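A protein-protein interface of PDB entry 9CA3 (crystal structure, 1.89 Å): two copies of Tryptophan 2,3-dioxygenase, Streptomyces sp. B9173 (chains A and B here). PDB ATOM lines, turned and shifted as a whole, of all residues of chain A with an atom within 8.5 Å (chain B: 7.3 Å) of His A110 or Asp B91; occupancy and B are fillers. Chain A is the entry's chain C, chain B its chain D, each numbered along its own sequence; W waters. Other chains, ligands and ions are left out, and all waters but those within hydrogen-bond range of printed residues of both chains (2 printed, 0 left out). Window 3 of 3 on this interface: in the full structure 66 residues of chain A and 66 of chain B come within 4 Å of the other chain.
Water W1 lies within hydrogen-bond range of NE of Arg B92, O of Arg B88 and O of His A110.
Water W2 lies within hydrogen-bond range of the backbone carbonyl oxygen (O) of Gly B95 and the side-chain amide oxygen (OE1) of Gln A102.
Arg B92 touches Phe A52.
Gly B95 touches Leu A106 (C to CD2, 3.5 Å).
CD2 of Leu B96 touches CD1 of Leu A106, 3.8 Å away.
Asp B91 touches His A110.
NH2 of Arg B92 touches CD of Pro A112 (3.8 Å).
Printed residues of chain B that touch a printed residue of chain A: Asp B91, Arg B92, Gly B95 and Leu B96.
Hydrophobic or aromatic side chains of chain B that line the printed part of chain A: Leu B96.
Printed residues of chain A that touch a printed residue of chain B: Asp A49, Phe A52, Leu A106, His A110 and Pro A112.
Among the printed residues, Asp or Glu carboxylates within 4 Å of a Lys or Arg side-chain nitrogen of the other chain: Asp A49 with Arg B92.
The side-chain hydroxyl of Ser A115 is in hydrogen-bond range of the side-chain carboxylate of Asp A49 (2.7 Å).
OD1 of Asp B91 is in salt-bridge range of NH2 of Arg B191 (2.8 Å).
No position is printed for both chains.
Of the 7 pairs that touch across the chains among the printed residues, none has its exchanged pair printed and touching as well.
The side-chain carboxylate (OD1) of Asp A49 is in salt-bridge range of the guanidinium group (NH1) of Arg B92 (3.0 Å).
NH2 of Arg B92 is in hydrogen-bond range of O of His A110 (3.3 Å).
His A110 touches just these residues of chain B: Asp B91 (3.5 Å) and Arg B92 (3.3 Å).
Of chain A, only His A110 (3.5 Å) comes within 4 Å of Asp B91.
Of the printed residues of chain B, Asp A49 touches Arg B92 (3.0 Å).
Of the printed residues of chain A, Leu B96 touches Leu A106 (3.8 Å).
Of the printed residues of chain B, Phe A52 touches Arg B92 (3.4 Å).
Of the printed residues of chain A, Gly B95 touches Leu A106.
Printed residues of chain B within 4 Å of Leu A106: Gly B95 and Leu B96.
Arg B191 touches none of the printed residues of chain A.
The nearest residue of chain B that does not touch His A110 is Gly B95 (4.7 Å).
The nearest printed residue of chain B that does not touch Phe A52 is Leu B96 (4.2 Å).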
ATOM      1  N   ASP A  49     -24.090   1.985 -14.221  1.00  0.00           N
ATOM      2  CA  ASP A  49     -22.810   2.062 -14.915  1.00  0.00           C
ATOM      3  C   ASP A  49     -21.757   1.123 -14.341  1.00  0.00           C
ATOM      4  O   ASP A  49     -20.646   1.062 -14.881  1.00  0.00           O
ATOM      5  CB  ASP A  49     -22.301   3.515 -14.914  1.00  0.00           C
ATOM      6  CG  ASP A  49     -23.143   4.404 -15.806  1.00  0.00           C
ATOM      7  OD1 ASP A  49     -23.640   3.886 -16.831  1.00  0.00           O
ATOM      8  OD2 ASP A  49     -23.349   5.590 -15.479  1.00  0.00           O
ATOM      9  N   PHE A  52     -20.457  -1.596 -16.994  1.00  0.00           N
ATOM     10  CA  PHE A  52     -19.552  -1.017 -17.984  1.00  0.00           C
ATOM     11  C   PHE A  52     -18.164  -0.818 -17.385  1.00  0.00           C
ATOM     12  O   PHE A  52     -17.159  -1.214 -17.975  1.00  0.00           O
ATOM     13  CB  PHE A  52     -20.161   0.295 -18.488  1.00  0.00           C
ATOM     14  CG  PHE A  52     -19.329   1.044 -19.478  1.00  0.00           C
ATOM     15  CD1 PHE A  52     -19.010   0.489 -20.710  1.00  0.00           C
ATOM     16  CD2 PHE A  52     -18.914   2.333 -19.202  1.00  0.00           C
ATOM     17  CE1 PHE A  52     -18.250   1.197 -21.646  1.00  0.00           C
ATOM     18  CE2 PHE A  52     -18.163   3.059 -20.135  1.00  0.00           C
ATOM     19  CZ  PHE A  52     -17.831   2.485 -21.351  1.00  0.00           C
ATOM     20  N   THR A  56     -14.761  -3.009 -18.828  1.00  0.00           N
ATOM     21  CA  THR A  56     -13.579  -2.411 -19.442  1.00  0.00           C
ATOM     22  C   THR A  56     -12.305  -2.864 -18.733  1.00  0.00           C
ATOM     23  O   THR A  56     -11.302  -3.128 -19.390  1.00  0.00           O
ATOM     24  CB  THR A  56     -13.660  -0.883 -19.482  1.00  0.00           C
ATOM     25  OG1 THR A  56     -13.683  -0.360 -18.146  1.00  0.00           O
ATOM     26  CG2 THR A  56     -14.904  -0.460 -20.232  1.00  0.00           C
ATOM     27  N   GLN A 102      -8.011   1.257 -26.332  1.00  0.00           N
ATOM     28  CA  GLN A 102      -9.398   1.522 -26.688  1.00  0.00           C
ATOM     29  C   GLN A 102     -10.326   1.267 -25.495  1.00  0.00           C
ATOM     30  O   GLN A 102     -11.329   1.975 -25.321  1.00  0.00           O
ATOM     31  CB  GLN A 102      -9.780   0.690 -27.942  1.00  0.00           C
ATOM     32  CG  GLN A 102     -10.426   1.624 -29.035  1.00  0.00           C
ATOM     33  CD  GLN A 102     -11.142   0.991 -30.278  1.00  0.00           C
ATOM     34  OE1 GLN A 102     -11.620  -0.161 -30.290  1.00  0.00           O
ATOM     35  NE2 GLN A 102     -11.235   1.814 -31.340  1.00  0.00           N
ATOM     36  N   ALA A 103      -9.975   0.323 -24.621  1.00  0.00           N
ATOM     37  CA  ALA A 103     -10.812   0.048 -23.453  1.00  0.00           C
ATOM     38  C   ALA A 103     -10.782   1.201 -22.453  1.00  0.00           C
ATOM     39  O   ALA A 103     -11.830   1.593 -21.917  1.00  0.00           O
ATOM     40  CB  ALA A 103     -10.364  -1.266 -22.783  1.00  0.00           C
ATOM     41  N   VAL A 104      -9.608   1.772 -22.177  1.00  0.00           N
ATOM     42  CA  VAL A 104      -9.608   2.856 -21.204  1.00  0.00           C
ATOM     43  C   VAL A 104     -10.288   4.086 -21.799  1.00  0.00           C
ATOM     44  O   VAL A 104     -10.974   4.830 -21.097  1.00  0.00           O
ATOM     45  CB  VAL A 104      -8.183   3.170 -20.709  1.00  0.00           C
ATOM     46  CG1 VAL A 104      -7.417   3.989 -21.741  1.00  0.00           C
ATOM     47  CG2 VAL A 104      -8.272   3.973 -19.410  1.00  0.00           C
ATOM     48  N   ARG A 105     -10.122   4.303 -23.106  1.00  0.00           N
ATOM     49  CA  ARG A 105     -10.721   5.442 -23.780  1.00  0.00           C
ATOM     50  C   ARG A 105     -12.236   5.324 -23.863  1.00  0.00           C
ATOM     51  O   ARG A 105     -12.916   6.347 -24.008  1.00  0.00           O
ATOM     52  CB  ARG A 105     -10.116   5.583 -25.181  1.00  0.00           C
ATOM     53  CG  ARG A 105      -8.645   5.964 -25.179  1.00  0.00           C
ATOM     54  CD  ARG A 105      -8.210   6.492 -26.560  1.00  0.00           C
ATOM     55  NE  ARG A 105      -8.935   7.729 -26.857  1.00  0.00           N
ATOM     56  CZ  ARG A 105      -8.842   8.401 -27.998  1.00  0.00           C
ATOM     57  NH1 ARG A 105      -8.029   8.011 -28.963  1.00  0.00           N
ATOM     58  NH2 ARG A 105      -9.569   9.504 -28.164  1.00  0.00           N
ATOM     59  N   LEU A 106     -12.768   4.096 -23.767  1.00  0.00           N
ATOM     60  CA  LEU A 106     -14.203   3.888 -23.610  1.00  0.00           C
ATOM     61  C   LEU A 106     -14.708   4.519 -22.329  1.00  0.00           C
ATOM     62  O   LEU A 106     -15.830   5.056 -22.282  1.00  0.00           O
ATOM     63  CB  LEU A 106     -14.511   2.396 -23.589  1.00  0.00           C
ATOM     64  CG  LEU A 106     -14.703   1.663 -24.901  1.00  0.00           C
ATOM     65  CD1 LEU A 106     -14.981   0.199 -24.581  1.00  0.00           C
ATOM     66  CD2 LEU A 106     -15.860   2.258 -25.673  1.00  0.00           C
ATOM     67  N   LEU A 107     -13.903   4.454 -21.262  1.00  0.00           N
ATOM     68  CA  LEU A 107     -14.289   5.160 -20.035  1.00  0.00           C
ATOM     69  C   LEU A 107     -14.216   6.667 -20.236  1.00  0.00           C
ATOM     70  O   LEU A 107     -15.111   7.417 -19.811  1.00  0.00           O
ATOM     71  CB  LEU A 107     -13.389   4.724 -18.878  1.00  0.00           C
ATOM     72  CG  LEU A 107     -13.528   3.260 -18.437  1.00  0.00           C
ATOM     73  CD1 LEU A 107     -12.794   3.006 -17.147  1.00  0.00           C
ATOM     74  CD2 LEU A 107     -14.963   2.887 -18.259  1.00  0.00           C
ATOM     75  N   THR A 108     -13.148   7.144 -20.872  1.00  0.00           N
ATOM     76  CA  THR A 108     -13.035   8.584 -21.070  1.00  0.00           C
ATOM     77  C   THR A 108     -14.217   9.113 -21.869  1.00  0.00           C
ATOM     78  O   THR A 108     -14.806  10.140 -21.521  1.00  0.00           O
ATOM     79  CB  THR A 108     -11.749   8.930 -21.795  1.00  0.00           C
ATOM     80  OG1 THR A 108     -10.626   8.372 -21.092  1.00  0.00           O
ATOM     81  CG2 THR A 108     -11.627  10.430 -21.867  1.00  0.00           C
ATOM     82  N   ASP A 109     -14.586   8.412 -22.931  1.00  0.00           N
ATOM     83  CA  ASP A 109     -15.634   8.910 -23.802  1.00  0.00           C
ATOM     84  C   ASP A 109     -17.043   8.671 -23.279  1.00  0.00           C
ATOM     85  O   ASP A 109     -17.954   9.403 -23.686  1.00  0.00           O
ATOM     86  CB  ASP A 109     -15.491   8.279 -25.200  1.00  0.00           C
ATOM     87  CG  ASP A 109     -14.197   8.654 -25.881  1.00  0.00           C
ATOM     88  OD1 ASP A 109     -13.595   9.699 -25.518  1.00  0.00           O
ATOM     89  OD2 ASP A 109     -13.784   7.913 -26.799  1.00  0.00           O
ATOM     90  N   HIS A 110     -17.264   7.683 -22.394  1.00  0.00           N
ATOM     91  CA  HIS A 110     -18.636   7.321 -22.010  1.00  0.00           C
ATOM     92  C   HIS A 110     -18.897   7.128 -20.522  1.00  0.00           C
ATOM     93  O   HIS A 110     -20.072   7.102 -20.135  1.00  0.00           O
ATOM     94  CB  HIS A 110     -19.083   6.043 -22.731  1.00  0.00           C
ATOM     95  CG  HIS A 110     -18.845   6.078 -24.207  1.00  0.00           C
ATOM     96  ND1 HIS A 110     -19.605   6.846 -25.065  1.00  0.00           N
ATOM     97  CD2 HIS A 110     -17.938   5.439 -24.977  1.00  0.00           C
ATOM     98  CE1 HIS A 110     -19.166   6.687 -26.301  1.00  0.00           C
ATOM     99  NE2 HIS A 110     -18.148   5.844 -26.272  1.00  0.00           N
ATOM    100  N   LEU A 111     -17.902   6.971 -19.669  1.00  0.00           N
ATOM    101  CA  LEU A 111     -18.199   6.831 -18.246  1.00  0.00           C
ATOM    102  C   LEU A 111     -18.557   8.195 -17.669  1.00  0.00           C
ATOM    103  O   LEU A 111     -17.711   9.096 -17.685  1.00  0.00           O
ATOM    104  CB  LEU A 111     -17.008   6.257 -17.489  1.00  0.00           C
ATOM    105  CG  LEU A 111     -17.254   6.053 -15.983  1.00  0.00           C
ATOM    106  CD1 LEU A 111     -18.330   5.004 -15.725  1.00  0.00           C
ATOM    107  CD2 LEU A 111     -15.925   5.655 -15.304  1.00  0.00           C
ATOM    108  N   PRO A 112     -19.764   8.386 -17.128  1.00  0.00           N
ATOM    109  CA  PRO A 112     -20.090   9.692 -16.520  1.00  0.00           C
ATOM    110  C   PRO A 112     -19.269   9.903 -15.257  1.00  0.00           C
ATOM    111  O   PRO A 112     -19.295   9.072 -14.340  1.00  0.00           O
ATOM    112  CB  PRO A 112     -21.588   9.590 -16.204  1.00  0.00           C
ATOM    113  CG  PRO A 112     -22.120   8.421 -17.006  1.00  0.00           C
ATOM    114  CD  PRO A 112     -20.912   7.463 -17.124  1.00  0.00           C
ATOM    115  N   GLN A 113     -18.545  11.024 -15.205  1.00  0.00           N
ATOM    116  CA  GLN A 113     -17.822  11.347 -13.976  1.00  0.00           C
ATOM    117  C   GLN A 113     -18.732  11.266 -12.759  1.00  0.00           C
ATOM    118  O   GLN A 113     -18.334  10.755 -11.707  1.00  0.00           O
ATOM    119  CB  GLN A 113     -17.187  12.738 -14.041  1.00  0.00           C
ATOM    120  CG  GLN A 113     -16.581  13.140 -12.679  1.00  0.00           C
ATOM    121  CD  GLN A 113     -16.018  14.542 -12.647  1.00  0.00           C
ATOM    122  OE1 GLN A 113     -16.530  15.440 -13.322  1.00  0.00           O
ATOM    123  NE2 GLN A 113     -14.960  14.747 -11.850  1.00  0.00           N
ATOM    124  N   SER A 115     -21.299   9.370 -12.162  1.00  0.00           N
ATOM    125  CA  SER A 115     -21.488   7.976 -11.757  1.00  0.00           C
ATOM    126  C   SER A 115     -20.234   7.421 -11.103  1.00  0.00           C
ATOM    127  O   SER A 115     -20.310   6.731 -10.079  1.00  0.00           O
ATOM    128  CB  SER A 115     -21.850   7.095 -12.960  1.00  0.00           C
ATOM    129  OG  SER A 115     -22.843   7.669 -13.770  1.00  0.00           O
ATOM    130  N   MET A 206      -8.029  10.252 -18.883  1.00  0.00           N
ATOM    131  CA  MET A 206      -9.215   9.734 -18.191  1.00  0.00           C
ATOM    132  C   MET A 206      -9.283  10.146 -16.722  1.00  0.00           C
ATOM    133  O   MET A 206     -10.314  10.661 -16.256  1.00  0.00           O
ATOM    134  CB  MET A 206      -9.209   8.227 -18.427  1.00  0.00           C
ATOM    135  CG  MET A 206     -10.201   7.202 -17.888  1.00  0.00           C
ATOM    136  SD  MET A 206     -10.441   7.298 -16.131  1.00  0.00           S
ATOM    137  CE  MET A 206      -9.205   6.012 -15.896  1.00  0.00           C
ATOM    138  N   SER A 209     -10.281  13.641 -16.177  1.00  0.00           N
ATOM    139  CA  SER A 209     -11.690  13.896 -16.447  1.00  0.00           C
ATOM    140  C   SER A 209     -12.624  13.289 -15.407  1.00  0.00           C
ATOM    141  O   SER A 209     -13.806  13.628 -15.392  1.00  0.00           O
ATOM    142  CB  SER A 209     -12.047  13.382 -17.849  1.00  0.00           C
ATOM    143  OG  SER A 209     -12.266  11.992 -17.870  1.00  0.00           O
ATOM    144  N   GLN A 210     -12.135  12.415 -14.535  1.00  0.00           N
ATOM    145  CA  GLN A 210     -12.978  11.759 -13.536  1.00  0.00           C
ATOM    146  C   GLN A 210     -12.723  12.230 -12.115  1.00  0.00           C
ATOM    147  O   GLN A 210     -13.665  12.321 -11.318  1.00  0.00           O
ATOM    148  CB  GLN A 210     -12.776  10.239 -13.608  1.00  0.00           C
ATOM    149  CG  GLN A 210     -13.148   9.634 -14.973  1.00  0.00           C
ATOM    150  CD  GLN A 210     -14.663   9.574 -15.154  1.00  0.00           C
ATOM    151  OE1 GLN A 210     -15.386   9.326 -14.201  1.00  0.00           O
ATOM    152  NE2 GLN A 210     -15.143   9.818 -16.369  1.00  0.00           N
ATOM    153  N   ALA B  86     -30.986   7.868 -24.030  1.00  0.00           N
ATOM    154  CA  ALA B  86     -30.857   6.750 -24.978  1.00  0.00           C
ATOM    155  C   ALA B  86     -29.657   6.927 -25.907  1.00  0.00           C
ATOM    156  O   ALA B  86     -28.998   5.944 -26.275  1.00  0.00           O
ATOM    157  CB  ALA B  86     -32.127   6.617 -25.806  1.00  0.00           C
ATOM    158  N   VAL B  87     -29.414   8.166 -26.357  1.00  0.00           N
ATOM    159  CA  VAL B  87     -28.270   8.456 -27.215  1.00  0.00           C
ATOM    160  C   VAL B  87     -26.994   7.868 -26.620  1.00  0.00           C
ATOM    161  O   VAL B  87     -26.245   7.152 -27.291  1.00  0.00           O
ATOM    162  CB  VAL B  87     -28.128   9.975 -27.430  1.00  0.00           C
ATOM    163  CG1 VAL B  87     -26.807  10.281 -28.170  1.00  0.00           C
ATOM    164  CG2 VAL B  87     -29.298  10.511 -28.197  1.00  0.00           C
ATOM    165  N   ARG B  88     -26.736   8.177 -25.348  1.00  0.00           N
ATOM    166  CA  ARG B  88     -25.515   7.738 -24.678  1.00  0.00           C
ATOM    167  C   ARG B  88     -25.385   6.220 -24.667  1.00  0.00           C
ATOM    168  O   ARG B  88     -24.276   5.692 -24.696  1.00  0.00           O
ATOM    169  CB  ARG B  88     -25.498   8.273 -23.245  1.00  0.00           C
ATOM    170  CG  ARG B  88     -25.477   9.786 -23.125  1.00  0.00           C
ATOM    171  CD  ARG B  88     -24.974  10.214 -21.763  1.00  0.00           C
ATOM    172  NE  ARG B  88     -25.181  11.651 -21.551  1.00  0.00           N
ATOM    173  CZ  ARG B  88     -26.263  12.197 -21.006  1.00  0.00           C
ATOM    174  NH1 ARG B  88     -27.279  11.452 -20.581  1.00  0.00           N
ATOM    175  NH2 ARG B  88     -26.335  13.530 -20.895  1.00  0.00           N
ATOM    176  N   MET B  89     -26.501   5.508 -24.594  1.00  0.00           N
ATOM    177  CA  MET B  89     -26.426   4.052 -24.569  1.00  0.00           C
ATOM    178  C   MET B  89     -25.959   3.533 -25.914  1.00  0.00           C
ATOM    179  O   MET B  89     -25.096   2.646 -25.987  1.00  0.00           O
ATOM    180  CB  MET B  89     -27.792   3.466 -24.264  1.00  0.00           C
ATOM    181  CG  MET B  89     -28.213   3.374 -22.824  1.00  0.00           C
ATOM    182  SD  MET B  89     -26.987   3.170 -21.547  1.00  0.00           S
ATOM    183  CE  MET B  89     -26.635   4.872 -21.176  1.00  0.00           C
ATOM    184  N   PHE B  90     -26.550   4.063 -26.993  1.00  0.00           N
ATOM    185  CA  PHE B  90     -26.156   3.684 -28.348  1.00  0.00           C
ATOM    186  C   PHE B  90     -24.692   4.025 -28.643  1.00  0.00           C
ATOM    187  O   PHE B  90     -23.966   3.197 -29.204  1.00  0.00           O
ATOM    188  CB  PHE B  90     -27.087   4.345 -29.364  1.00  0.00           C
ATOM    189  CG  PHE B  90     -28.483   3.796 -29.364  1.00  0.00           C
ATOM    190  CD1 PHE B  90     -28.708   2.433 -29.581  1.00  0.00           C
ATOM    191  CD2 PHE B  90     -29.579   4.619 -29.093  1.00  0.00           C
ATOM    192  CE1 PHE B  90     -29.992   1.905 -29.587  1.00  0.00           C
ATOM    193  CE2 PHE B  90     -30.895   4.093 -29.080  1.00  0.00           C
ATOM    194  CZ  PHE B  90     -31.087   2.724 -29.336  1.00  0.00           C
ATOM    195  N   ASP B  91     -24.228   5.227 -28.273  1.00  0.00           N
ATOM    196  CA  ASP B  91     -22.833   5.580 -28.542  1.00  0.00           C
ATOM    197  C   ASP B  91     -21.870   4.655 -27.804  1.00  0.00           C
ATOM    198  O   ASP B  91     -20.799   4.306 -28.321  1.00  0.00           O
ATOM    199  CB  ASP B  91     -22.551   7.026 -28.144  1.00  0.00           C
ATOM    200  CG  ASP B  91     -23.149   8.038 -29.111  1.00  0.00           C
ATOM    201  OD1 ASP B  91     -23.457   7.706 -30.286  1.00  0.00           O
ATOM    202  OD2 ASP B  91     -23.338   9.173 -28.662  1.00  0.00           O
ATOM    203  N   ARG B  92     -22.214   4.288 -26.576  1.00  0.00           N
ATOM    204  CA  ARG B  92     -21.397   3.359 -25.806  1.00  0.00           C
ATOM    205  C   ARG B  92     -21.362   1.975 -26.451  1.00  0.00           C
ATOM    206  O   ARG B  92     -20.293   1.343 -26.553  1.00  0.00           O
ATOM    207  CB  ARG B  92     -21.962   3.291 -24.386  1.00  0.00           C
ATOM    208  CG  ARG B  92     -21.039   2.723 -23.342  1.00  0.00           C
ATOM    209  CD  ARG B  92     -21.840   2.518 -22.070  1.00  0.00           C
ATOM    210  NE  ARG B  92     -22.037   3.754 -21.324  1.00  0.00           N
ATOM    211  CZ  ARG B  92     -22.309   3.793 -20.027  1.00  0.00           C
ATOM    212  NH1 ARG B  92     -22.392   2.681 -19.308  1.00  0.00           N
ATOM    213  NH2 ARG B  92     -22.556   4.972 -19.448  1.00  0.00           N
ATOM    214  N   ALA B  93     -22.528   1.473 -26.882  1.00  0.00           N
ATOM    215  CA  ALA B  93     -22.550   0.196 -27.574  1.00  0.00           C
ATOM    216  C   ALA B  93     -21.679   0.241 -28.812  1.00  0.00           C
ATOM    217  O   ALA B  93     -21.017  -0.746 -29.141  1.00  0.00           O
ATOM    218  CB  ALA B  93     -23.977  -0.189 -27.953  1.00  0.00           C
ATOM    219  N   THR B  94     -21.697   1.362 -29.531  1.00  0.00           N
ATOM    220  CA  THR B  94     -20.864   1.491 -30.714  1.00  0.00           C
ATOM    221  C   THR B  94     -19.383   1.376 -30.346  1.00  0.00           C
ATOM    222  O   THR B  94     -18.634   0.631 -30.981  1.00  0.00           O
ATOM    223  CB  THR B  94     -21.177   2.819 -31.419  1.00  0.00           C
ATOM    224  OG1 THR B  94     -22.530   2.801 -31.876  1.00  0.00           O
ATOM    225  CG2 THR B  94     -20.270   3.042 -32.618  1.00  0.00           C
ATOM    226  N   GLY B  95     -18.952   2.065 -29.282  1.00  0.00           N
ATOM    227  CA  GLY B  95     -17.564   1.939 -28.858  1.00  0.00           C
ATOM    228  C   GLY B  95     -17.197   0.522 -28.443  1.00  0.00           C
ATOM    229  O   GLY B  95     -16.094   0.046 -28.736  1.00  0.00           O
ATOM    230  N   LEU B  96     -18.101  -0.157 -27.741  1.00  0.00           N
ATOM    231  CA  LEU B  96     -17.902  -1.557 -27.380  1.00  0.00           C
ATOM    232  C   LEU B  96     -17.880  -2.448 -28.616  1.00  0.00           C
ATOM    233  O   LEU B  96     -17.094  -3.412 -28.689  1.00  0.00           O
ATOM    234  CB  LEU B  96     -19.000  -1.999 -26.418  1.00  0.00           C
ATOM    235  CG  LEU B  96     -18.860  -1.404 -25.019  1.00  0.00           C
ATOM    236  CD1 LEU B  96     -20.237  -1.366 -24.319  1.00  0.00           C
ATOM    237  CD2 LEU B  96     -17.890  -2.253 -24.229  1.00  0.00           C
ATOM    238  N   SER B  97     -18.717  -2.129 -29.612  1.00  0.00           N
ATOM    239  CA  SER B  97     -18.676  -2.884 -30.859  1.00  0.00           C
ATOM    240  C   SER B  97     -17.329  -2.707 -31.567  1.00  0.00           C
ATOM    241  O   SER B  97     -16.776  -3.671 -32.107  1.00  0.00           O
ATOM    242  CB  SER B  97     -19.824  -2.465 -31.781  1.00  0.00           C
ATOM    243  OG  SER B  97     -19.712  -3.079 -33.067  1.00  0.00           O
ATOM    244  N   LEU B 184     -30.782  12.608 -33.204  1.00  0.00           N
ATOM    245  CA  LEU B 184     -29.510  12.153 -32.643  1.00  0.00           C
ATOM    246  C   LEU B 184     -29.570  10.677 -32.268  1.00  0.00           C
ATOM    247  O   LEU B 184     -28.549   9.972 -32.330  1.00  0.00           O
ATOM    248  CB  LEU B 184     -29.159  12.981 -31.402  1.00  0.00           C
ATOM    249  CG  LEU B 184     -28.913  14.478 -31.558  1.00  0.00           C
ATOM    250  CD1 LEU B 184     -28.577  15.133 -30.215  1.00  0.00           C
ATOM    251  CD2 LEU B 184     -27.802  14.722 -32.578  1.00  0.00           C
ATOM    252  N   VAL B 185     -30.742  10.197 -31.853  1.00  0.00           N
ATOM    253  CA  VAL B 185     -30.889   8.778 -31.542  1.00  0.00           C
ATOM    254  C   VAL B 185     -30.787   7.954 -32.818  1.00  0.00           C
ATOM    255  O   VAL B 185     -30.074   6.936 -32.860  1.00  0.00           O
ATOM    256  CB  VAL B 185     -32.215   8.503 -30.801  1.00  0.00           C
ATOM    257  CG1 VAL B 185     -32.430   6.991 -30.617  1.00  0.00           C
ATOM    258  CG2 VAL B 185     -32.284   9.254 -29.461  1.00  0.00           C
ATOM    259  N   GLU B 187     -29.210   8.723 -35.557  1.00  0.00           N
ATOM    260  CA  GLU B 187     -27.832   8.757 -36.022  1.00  0.00           C
ATOM    261  C   GLU B 187     -26.956   7.812 -35.205  1.00  0.00           C
ATOM    262  O   GLU B 187     -26.143   7.079 -35.773  1.00  0.00           O
ATOM    263  CB  GLU B 187     -27.323  10.196 -36.011  1.00  0.00           C
ATOM    264  CG  GLU B 187     -28.151  11.078 -36.954  1.00  0.00           C
ATOM    265  CD  GLU B 187     -28.250  12.548 -36.532  1.00  0.00           C
ATOM    266  OE1 GLU B 187     -27.314  13.076 -35.887  1.00  0.00           O
ATOM    267  OE2 GLU B 187     -29.298  13.174 -36.833  1.00  0.00           O
ATOM    268  N   ALA B 188     -27.167   7.758 -33.889  1.00  0.00           N
ATOM    269  CA  ALA B 188     -26.408   6.849 -33.035  1.00  0.00           C
ATOM    270  C   ALA B 188     -26.746   5.386 -33.295  1.00  0.00           C
ATOM    271  O   ALA B 188     -25.855   4.520 -33.220  1.00  0.00           O
ATOM    272  CB  ALA B 188     -26.644   7.173 -31.566  1.00  0.00           C
ATOM    273  N   MET B 189     -28.015   5.056 -33.551  1.00  0.00           N
ATOM    274  CA  MET B 189     -28.270   3.656 -33.888  1.00  0.00           C
ATOM    275  C   MET B 189     -27.770   3.289 -35.276  1.00  0.00           C
ATOM    276  O   MET B 189     -27.387   2.138 -35.490  1.00  0.00           O
ATOM    277  CB  MET B 189     -29.745   3.203 -33.684  1.00  0.00           C
ATOM    278  CG  MET B 189     -30.616   3.866 -32.640  1.00  0.00           C
ATOM    279  SD  MET B 189     -32.422   3.845 -32.916  1.00  0.00           S
ATOM    280  CE  MET B 189     -32.750   2.132 -32.527  1.00  0.00           C
ATOM    281  N   ARG B 191     -24.880   4.492 -36.527  1.00  0.00           N
ATOM    282  CA  ARG B 191     -23.458   4.266 -36.288  1.00  0.00           C
ATOM    283  C   ARG B 191     -23.221   2.900 -35.658  1.00  0.00           C
ATOM    284  O   ARG B 191     -22.282   2.193 -36.038  1.00  0.00           O
ATOM    285  CB  ARG B 191     -22.872   5.388 -35.413  1.00  0.00           C
ATOM    286  CG  ARG B 191     -22.616   6.697 -36.184  1.00  0.00           C
ATOM    287  CD  ARG B 191     -21.880   7.797 -35.352  1.00  0.00           C
ATOM    288  NE  ARG B 191     -22.523   8.070 -34.064  1.00  0.00           N
ATOM    289  CZ  ARG B 191     -23.441   9.008 -33.865  1.00  0.00           C
ATOM    290  NH1 ARG B 191     -23.845   9.797 -34.849  1.00  0.00           N
ATOM    291  NH2 ARG B 191     -23.962   9.168 -32.645  1.00  0.00           N
ATOM    292  N   LEU B 192     -24.069   2.501 -34.702  1.00  0.00           N
ATOM    293  CA  LEU B 192     -23.930   1.178 -34.100  1.00  0.00           C
ATOM    294  C   LEU B 192     -24.077   0.079 -35.148  1.00  0.00           C
ATOM    295  O   LEU B 192     -23.299  -0.888 -35.186  1.00  0.00           O
ATOM    296  CB  LEU B 192     -24.983   1.004 -33.004  1.00  0.00           C
ATOM    297  CG  LEU B 192     -25.109  -0.374 -32.360  1.00  0.00           C
ATOM    298  CD1 LEU B 192     -23.770  -0.862 -31.814  1.00  0.00           C
ATOM    299  CD2 LEU B 192     -26.160  -0.314 -31.243  1.00  0.00           C
HETATM  300  O   HOH W   1     -22.595   6.300 -22.315  1.00  0.00           O
HETATM  301  O   HOH W   2     -13.824   1.647 -29.021  1.00  0.00           O
